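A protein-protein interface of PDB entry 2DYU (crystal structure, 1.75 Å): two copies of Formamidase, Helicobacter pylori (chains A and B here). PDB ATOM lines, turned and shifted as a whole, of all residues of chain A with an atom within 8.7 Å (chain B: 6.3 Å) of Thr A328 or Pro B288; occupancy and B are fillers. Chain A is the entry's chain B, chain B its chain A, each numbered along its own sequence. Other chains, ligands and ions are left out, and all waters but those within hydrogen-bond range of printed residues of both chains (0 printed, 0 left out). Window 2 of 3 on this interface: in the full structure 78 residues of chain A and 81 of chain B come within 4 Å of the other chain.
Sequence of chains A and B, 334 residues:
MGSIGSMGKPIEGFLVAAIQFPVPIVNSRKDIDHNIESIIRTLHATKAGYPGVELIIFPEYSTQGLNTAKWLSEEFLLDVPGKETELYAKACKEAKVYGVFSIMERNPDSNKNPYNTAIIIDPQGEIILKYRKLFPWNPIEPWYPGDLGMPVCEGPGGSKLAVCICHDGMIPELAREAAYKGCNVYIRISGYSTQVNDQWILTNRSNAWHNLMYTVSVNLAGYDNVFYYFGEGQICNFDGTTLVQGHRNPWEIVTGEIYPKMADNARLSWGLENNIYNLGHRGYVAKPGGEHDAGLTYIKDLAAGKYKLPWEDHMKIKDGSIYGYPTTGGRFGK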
ATOM      1  N   LYS A 112      19.918   6.891  -6.706  1.00  0.00           N
ATOM      2  CA  LYS A 112      21.238   6.416  -6.295  1.00  0.00           C
ATOM      3  C   LYS A 112      21.350   4.893  -6.225  1.00  0.00           C
ATOM      4  O   LYS A 112      20.356   4.194  -6.005  1.00  0.00           O
ATOM      5  CB  LYS A 112      21.598   6.985  -4.921  1.00  0.00           C
ATOM      6  CG  LYS A 112      21.690   8.495  -4.829  1.00  0.00           C
ATOM      7  CD  LYS A 112      22.156   8.883  -3.434  1.00  0.00           C
ATOM      8  CE  LYS A 112      22.293  10.384  -3.272  1.00  0.00           C
ATOM      9  NZ  LYS A 112      22.978  10.714  -1.990  1.00  0.00           N
ATOM     10  N   TYR A 144      26.906   2.505  -3.155  1.00  0.00           N
ATOM     11  CA  TYR A 144      27.058   3.931  -2.924  1.00  0.00           C
ATOM     12  C   TYR A 144      27.814   4.166  -1.618  1.00  0.00           C
ATOM     13  O   TYR A 144      27.573   3.466  -0.636  1.00  0.00           O
ATOM     14  CB  TYR A 144      25.678   4.595  -2.868  1.00  0.00           C
ATOM     15  CG  TYR A 144      25.694   6.062  -3.229  1.00  0.00           C
ATOM     16  CD1 TYR A 144      25.601   6.470  -4.555  1.00  0.00           C
ATOM     17  CD2 TYR A 144      25.809   7.038  -2.249  1.00  0.00           C
ATOM     18  CE1 TYR A 144      25.621   7.813  -4.894  1.00  0.00           C
ATOM     19  CE2 TYR A 144      25.833   8.384  -2.578  1.00  0.00           C
ATOM     20  CZ  TYR A 144      25.737   8.765  -3.903  1.00  0.00           C
ATOM     21  OH  TYR A 144      25.756  10.104  -4.239  1.00  0.00           O
ATOM     22  N   PRO A 145      28.746   5.139  -1.610  1.00  0.00           N
ATOM     23  CA  PRO A 145      29.466   5.534  -0.394  1.00  0.00           C
ATOM     24  C   PRO A 145      28.523   5.795   0.784  1.00  0.00           C
ATOM     25  O   PRO A 145      27.560   6.556   0.653  1.00  0.00           O
ATOM     26  CB  PRO A 145      30.163   6.832  -0.808  1.00  0.00           C
ATOM     27  CG  PRO A 145      30.349   6.703  -2.275  1.00  0.00           C
ATOM     28  CD  PRO A 145      29.186   5.908  -2.788  1.00  0.00           C
ATOM     29  N   LYS A 318      41.096   4.895 -11.610  1.00  0.00           N
ATOM     30  CA  LYS A 318      40.359   5.965 -10.939  1.00  0.00           C
ATOM     31  C   LYS A 318      38.860   5.923 -11.255  1.00  0.00           C
ATOM     32  O   LYS A 318      38.080   6.691 -10.689  1.00  0.00           O
ATOM     33  CB  LYS A 318      40.944   7.340 -11.287  1.00  0.00           C
ATOM     34  CG  LYS A 318      42.174   7.723 -10.470  1.00  0.00           C
ATOM     35  CD  LYS A 318      42.563   9.182 -10.669  1.00  0.00           C
ATOM     36  CE  LYS A 318      43.169   9.425 -12.043  1.00  0.00           C
ATOM     37  NZ  LYS A 318      43.692  10.815 -12.173  1.00  0.00           N
ATOM     38  N   ASP A 319      38.468   5.033 -12.166  1.00  0.00           N
ATOM     39  CA  ASP A 319      37.052   4.779 -12.459  1.00  0.00           C
ATOM     40  C   ASP A 319      36.827   3.318 -12.858  1.00  0.00           C
ATOM     41  O   ASP A 319      37.756   2.638 -13.301  1.00  0.00           O
ATOM     42  CB  ASP A 319      36.506   5.753 -13.517  1.00  0.00           C
ATOM     43  CG  ASP A 319      37.071   5.502 -14.905  1.00  0.00           C
ATOM     44  OD1 ASP A 319      36.563   4.601 -15.606  1.00  0.00           O
ATOM     45  OD2 ASP A 319      38.006   6.226 -15.307  1.00  0.00           O
ATOM     46  N   GLY A 320      35.591   2.845 -12.704  1.00  0.00           N
ATOM     47  CA  GLY A 320      35.284   1.421 -12.853  1.00  0.00           C
ATOM     48  C   GLY A 320      34.867   0.946 -14.234  1.00  0.00           C
ATOM     49  O   GLY A 320      33.927   0.160 -14.366  1.00  0.00           O
ATOM     50  N   TYR A 325      31.247   0.155 -15.306  1.00  0.00           N
ATOM     51  CA  TYR A 325      30.471   1.045 -14.441  1.00  0.00           C
ATOM     52  C   TYR A 325      30.439   2.483 -14.964  1.00  0.00           C
ATOM     53  O   TYR A 325      31.484   3.057 -15.278  1.00  0.00           O
ATOM     54  CB  TYR A 325      31.023   1.041 -13.011  1.00  0.00           C
ATOM     55  CG  TYR A 325      30.769  -0.234 -12.238  1.00  0.00           C
ATOM     56  CD1 TYR A 325      29.475  -0.631 -11.922  1.00  0.00           C
ATOM     57  CD2 TYR A 325      31.823  -1.032 -11.810  1.00  0.00           C
ATOM     58  CE1 TYR A 325      29.235  -1.795 -11.214  1.00  0.00           C
ATOM     59  CE2 TYR A 325      31.593  -2.197 -11.099  1.00  0.00           C
ATOM     60  CZ  TYR A 325      30.296  -2.573 -10.803  1.00  0.00           C
ATOM     61  OH  TYR A 325      30.056  -3.730 -10.098  1.00  0.00           O
ATOM     62  N   PRO A 326      29.230   3.064 -15.068  1.00  0.00           N
ATOM     63  CA  PRO A 326      29.052   4.485 -15.364  1.00  0.00           C
ATOM     64  C   PRO A 326      29.418   5.344 -14.150  1.00  0.00           C
ATOM     65  O   PRO A 326      28.729   5.302 -13.127  1.00  0.00           O
ATOM     66  CB  PRO A 326      27.548   4.600 -15.667  1.00  0.00           C
ATOM     67  CG  PRO A 326      27.048   3.186 -15.805  1.00  0.00           C
ATOM     68  CD  PRO A 326      27.939   2.371 -14.934  1.00  0.00           C
ATOM     69  N   THR A 327      30.495   6.117 -14.273  1.00  0.00           N
ATOM     70  CA  THR A 327      31.018   6.893 -13.149  1.00  0.00           C
ATOM     71  C   THR A 327      30.703   8.390 -13.244  1.00  0.00           C
ATOM     72  O   THR A 327      31.132   9.175 -12.394  1.00  0.00           O
ATOM     73  CB  THR A 327      32.542   6.690 -12.983  1.00  0.00           C
ATOM     74  OG1 THR A 327      33.215   7.084 -14.186  1.00  0.00           O
ATOM     75  CG2 THR A 327      32.858   5.230 -12.690  1.00  0.00           C
ATOM     76  N   THR A 328      29.957   8.776 -14.278  1.00  0.00           N
ATOM     77  CA  THR A 328      29.524  10.164 -14.445  1.00  0.00           C
ATOM     78  C   THR A 328      28.380  10.473 -13.478  1.00  0.00           C
ATOM     79  O   THR A 328      28.264  11.590 -12.969  1.00  0.00           O
ATOM     80  CB  THR A 328      29.070  10.455 -15.899  1.00  0.00           C
ATOM     81  OG1 THR A 328      29.996   9.871 -16.824  1.00  0.00           O
ATOM     82  CG2 THR A 328      28.985  11.955 -16.156  1.00  0.00           C
ATOM     83  N   GLY A 329      27.547   9.466 -13.225  1.00  0.00           N
ATOM     84  CA  GLY A 329      26.404   9.599 -12.327  1.00  0.00           C
ATOM     85  C   GLY A 329      25.270   8.672 -12.728  1.00  0.00           C
ATOM     86  O   GLY A 329      25.503   7.610 -13.309  1.00  0.00           O
ATOM     87  N   GLY A 330      24.042   9.073 -12.411  1.00  0.00           N
ATOM     88  CA  GLY A 330      22.852   8.320 -12.805  1.00  0.00           C
ATOM     89  C   GLY A 330      22.629   7.029 -12.038  1.00  0.00           C
ATOM     90  O   GLY A 330      23.274   6.777 -11.018  1.00  0.00           O
ATOM     91  N   ARG A 331      21.705   6.212 -12.538  1.00  0.00           N
ATOM     92  CA  ARG A 331      21.363   4.935 -11.918  1.00  0.00           C
ATOM     93  C   ARG A 331      21.513   3.802 -12.932  1.00  0.00           C
ATOM     94  O   ARG A 331      21.136   3.948 -14.096  1.00  0.00           O
ATOM     95  CB  ARG A 331      19.930   4.978 -11.378  1.00  0.00           C
ATOM     96  CG  ARG A 331      19.478   3.727 -10.634  1.00  0.00           C
ATOM     97  CD  ARG A 331      20.270   3.502  -9.359  1.00  0.00           C
ATOM     98  NE  ARG A 331      19.652   2.491  -8.504  1.00  0.00           N
ATOM     99  CZ  ARG A 331      19.933   1.192  -8.551  1.00  0.00           C
ATOM    100  NH1 ARG A 331      20.828   0.732  -9.415  1.00  0.00           N
ATOM    101  NH2 ARG A 331      19.318   0.349  -7.732  1.00  0.00           N
ATOM    102  N   PHE A 332      22.063   2.677 -12.484  1.00  0.00           N
ATOM    103  CA  PHE A 332      22.326   1.546 -13.373  1.00  0.00           C
ATOM    104  C   PHE A 332      22.222   0.195 -12.665  1.00  0.00           C
ATOM    105  O   PHE A 332      22.477   0.091 -11.464  1.00  0.00           O
ATOM    106  CB  PHE A 332      23.704   1.692 -14.033  1.00  0.00           C
ATOM    107  CG  PHE A 332      24.832   1.904 -13.057  1.00  0.00           C
ATOM    108  CD1 PHE A 332      25.529   0.823 -12.535  1.00  0.00           C
ATOM    109  CD2 PHE A 332      25.200   3.185 -12.667  1.00  0.00           C
ATOM    110  CE1 PHE A 332      26.565   1.016 -11.639  1.00  0.00           C
ATOM    111  CE2 PHE A 332      26.239   3.384 -11.773  1.00  0.00           C
ATOM    112  CZ  PHE A 332      26.924   2.297 -11.261  1.00  0.00           C
ATOM    113  N   GLY B 283      34.402   6.050  -3.028  1.00  0.00           N
ATOM    114  CA  GLY B 283      33.404   5.606  -3.998  1.00  0.00           C
ATOM    115  C   GLY B 283      33.285   6.470  -5.239  1.00  0.00           C
ATOM    116  O   GLY B 283      32.277   7.151  -5.435  1.00  0.00           O
ATOM    117  N   TYR B 284      34.315   6.437  -6.081  1.00  0.00           N
ATOM    118  CA  TYR B 284      34.299   7.161  -7.354  1.00  0.00           C
ATOM    119  C   TYR B 284      33.453   6.451  -8.421  1.00  0.00           C
ATOM    120  O   TYR B 284      33.135   7.031  -9.464  1.00  0.00           O
ATOM    121  CB  TYR B 284      35.729   7.398  -7.860  1.00  0.00           C
ATOM    122  CG  TYR B 284      36.660   6.212  -7.700  1.00  0.00           C
ATOM    123  CD1 TYR B 284      36.555   5.098  -8.533  1.00  0.00           C
ATOM    124  CD2 TYR B 284      37.650   6.208  -6.722  1.00  0.00           C
ATOM    125  CE1 TYR B 284      37.410   4.011  -8.395  1.00  0.00           C
ATOM    126  CE2 TYR B 284      38.510   5.124  -6.574  1.00  0.00           C
ATOM    127  CZ  TYR B 284      38.384   4.029  -7.414  1.00  0.00           C
ATOM    128  OH  TYR B 284      39.232   2.950  -7.273  1.00  0.00           O
ATOM    129  N   VAL B 285      33.091   5.199  -8.145  1.00  0.00           N
ATOM    130  CA  VAL B 285      32.311   4.381  -9.075  1.00  0.00           C
ATOM    131  C   VAL B 285      30.806   4.640  -8.947  1.00  0.00           C
ATOM    132  O   VAL B 285      30.083   4.657  -9.946  1.00  0.00           O
ATOM    133  CB  VAL B 285      32.627   2.870  -8.892  1.00  0.00           C
ATOM    134  CG1 VAL B 285      31.565   1.996  -9.548  1.00  0.00           C
ATOM    135  CG2 VAL B 285      34.009   2.545  -9.446  1.00  0.00           C
ATOM    136  N   ALA B 286      30.342   4.850  -7.717  1.00  0.00           N
ATOM    137  CA  ALA B 286      28.929   5.126  -7.471  1.00  0.00           C
ATOM    138  C   ALA B 286      28.656   6.628  -7.400  1.00  0.00           C
ATOM    139  O   ALA B 286      27.719   7.127  -8.027  1.00  0.00           O
ATOM    140  CB  ALA B 286      28.463   4.432  -6.202  1.00  0.00           C
ATOM    141  N   LYS B 287      29.476   7.340  -6.632  1.00  0.00           N
ATOM    142  CA  LYS B 287      29.396   8.796  -6.561  1.00  0.00           C
ATOM    143  C   LYS B 287      30.381   9.399  -7.563  1.00  0.00           C
ATOM    144  O   LYS B 287      31.522   8.943  -7.655  1.00  0.00           O
ATOM    145  CB  LYS B 287      29.696   9.281  -5.138  1.00  0.00           C
ATOM    146  CG  LYS B 287      29.401  10.756  -4.897  1.00  0.00           C
ATOM    147  CD  LYS B 287      29.365  11.080  -3.412  1.00  0.00           C
ATOM    148  CE  LYS B 287      29.141  12.570  -3.171  1.00  0.00           C
ATOM    149  NZ  LYS B 287      27.791  13.022  -3.612  1.00  0.00           N
ATOM    150  N   PRO B 288      29.939  10.415  -8.329  1.00  0.00           N
ATOM    151  CA  PRO B 288      30.799  11.035  -9.340  1.00  0.00           C
ATOM    152  C   PRO B 288      32.089  11.595  -8.741  1.00  0.00           C
ATOM    153  O   PRO B 288      32.055  12.594  -8.018  1.00  0.00           O
ATOM    154  CB  PRO B 288      29.933  12.174  -9.892  1.00  0.00           C
ATOM    155  CG  PRO B 288      28.530  11.771  -9.591  1.00  0.00           C
ATOM    156  CD  PRO B 288      28.599  11.032  -8.292  1.00  0.00           C
ATOM    157  N   GLY B 289      33.211  10.942  -9.035  1.00  0.00           N
ATOM    158  CA  GLY B 289      34.516  11.365  -8.523  1.00  0.00           C
ATOM    159  C   GLY B 289      34.821  10.822  -7.137  1.00  0.00           C
ATOM    160  O   GLY B 289      35.985  10.625  -6.776  1.00  0.00           O
ATOM    161  N   GLY B 290      33.769  10.580  -6.359  1.00  0.00           N
ATOM    162  CA  GLY B 290      33.911  10.078  -4.997  1.00  0.00           C
ATOM    163  C   GLY B 290      33.657  11.148  -3.952  1.00  0.00           C
ATOM    164  O   GLY B 290      33.917  12.331  -4.184  1.00  0.00           O
ATOM    165  N   GLU B 291      33.139  10.734  -2.799  1.00  0.00           N
ATOM    166  CA  GLU B 291      32.914  11.658  -1.693  1.00  0.00           C
ATOM    167  C   GLU B 291      34.227  11.931  -0.963  1.00  0.00           C
ATOM    168  O   GLU B 291      35.050  11.030  -0.790  1.00  0.00           O
ATOM    169  CB  GLU B 291      31.857  11.109  -0.728  1.00  0.00           C
ATOM    170  CG  GLU B 291      31.599  11.967   0.515  1.00  0.00           C
ATOM    171  CD  GLU B 291      30.976  13.324   0.208  1.00  0.00           C
ATOM    172  OE1 GLU B 291      29.830  13.561   0.646  1.00  0.00           O
ATOM    173  OE2 GLU B 291      31.628  14.156  -0.463  1.00  0.00           O
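Printed residues of chain A that touch a printed residue of chain B: Tyr A144, Pro A145, Lys A318, Asp A319, Gly A320, Tyr A325, Pro A326, Thr A327 and Thr A328.
Hydrophobic or aromatic side chains of chain A within 4 Å of the printed part of chain B: Tyr A144, Pro A145 and Tyr A325.
Of the 9 printed residues of chain B, 6 touch a printed residue of chain A.
Hydrophobic or aromatic side chains of chain B that line the printed part of chain A: Tyr B284, Val B285, Ala B286 and Pro B288.
Among the printed residues, 14 pairs touch across the chains.
Among the printed residues, no Asp or Glu carboxylate lies within 4 Å of a Lys or Arg side-chain nitrogen of the other chain.
Lys A112 touches none of the printed residues of chain B.
Printed residues of chain B within 4 Å of Tyr A144: Ala B286 and Lys B287.
Of the printed residues of chain B, Lys A318 touches Tyr B284 (3.1 Å).
Printed residues of chain B within 4 Å of Asp A319: Tyr B284.
Of chain B, only Pro B288 (3.4 Å) comes within 4 Å of Thr A328.
Printed residues of chain A within 4 Å of Gly B283: Pro A145 (3.7 Å).
Printed residues of chain A within 4 Å of Lys B287: Tyr A144 (3.6 Å) and Pro A145 (3.9 Å).
Of chain A, only Thr A327 and Thr A328 come within 4 Å of Pro B288.
No residue of chain A comes within 4 Å of Gly B289.
No residue of chain A comes within 4 Å of Gly B290.
Glu B291 touches none of the printed residues of chain A.
The nearest printed residue of chain A that does not touch Ala B286 is Gly A329 (5.1 Å).
Among the printed residues, merely in contact across the chains: Lys A318 with Tyr B284, Thr A328 with Pro B288, Pro A326 with Val B285, Tyr A325 with Val B285, Thr A327 with Tyr B284, Thr A327 with Pro B288, Tyr A144 with Ala B286, Tyr A144 with Lys B287, Gly A320 with Val B285, Pro A145 with Gly B283, Thr A327 with Val B285, Pro A145 with Ala B286, Pro A145 with Lys B287 and Asp A319 with Tyr B284.
The backbone NH (N) of Tyr A325 sits at hydrogen-bond distance from the backbone carbonyl oxygen (O) of Gly A320, at 2.8 Å.
No position is printed for both chains.
Of the 14 pairs that touch across the chains among the printed residues, none has its exchanged pair printed and touching as well.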
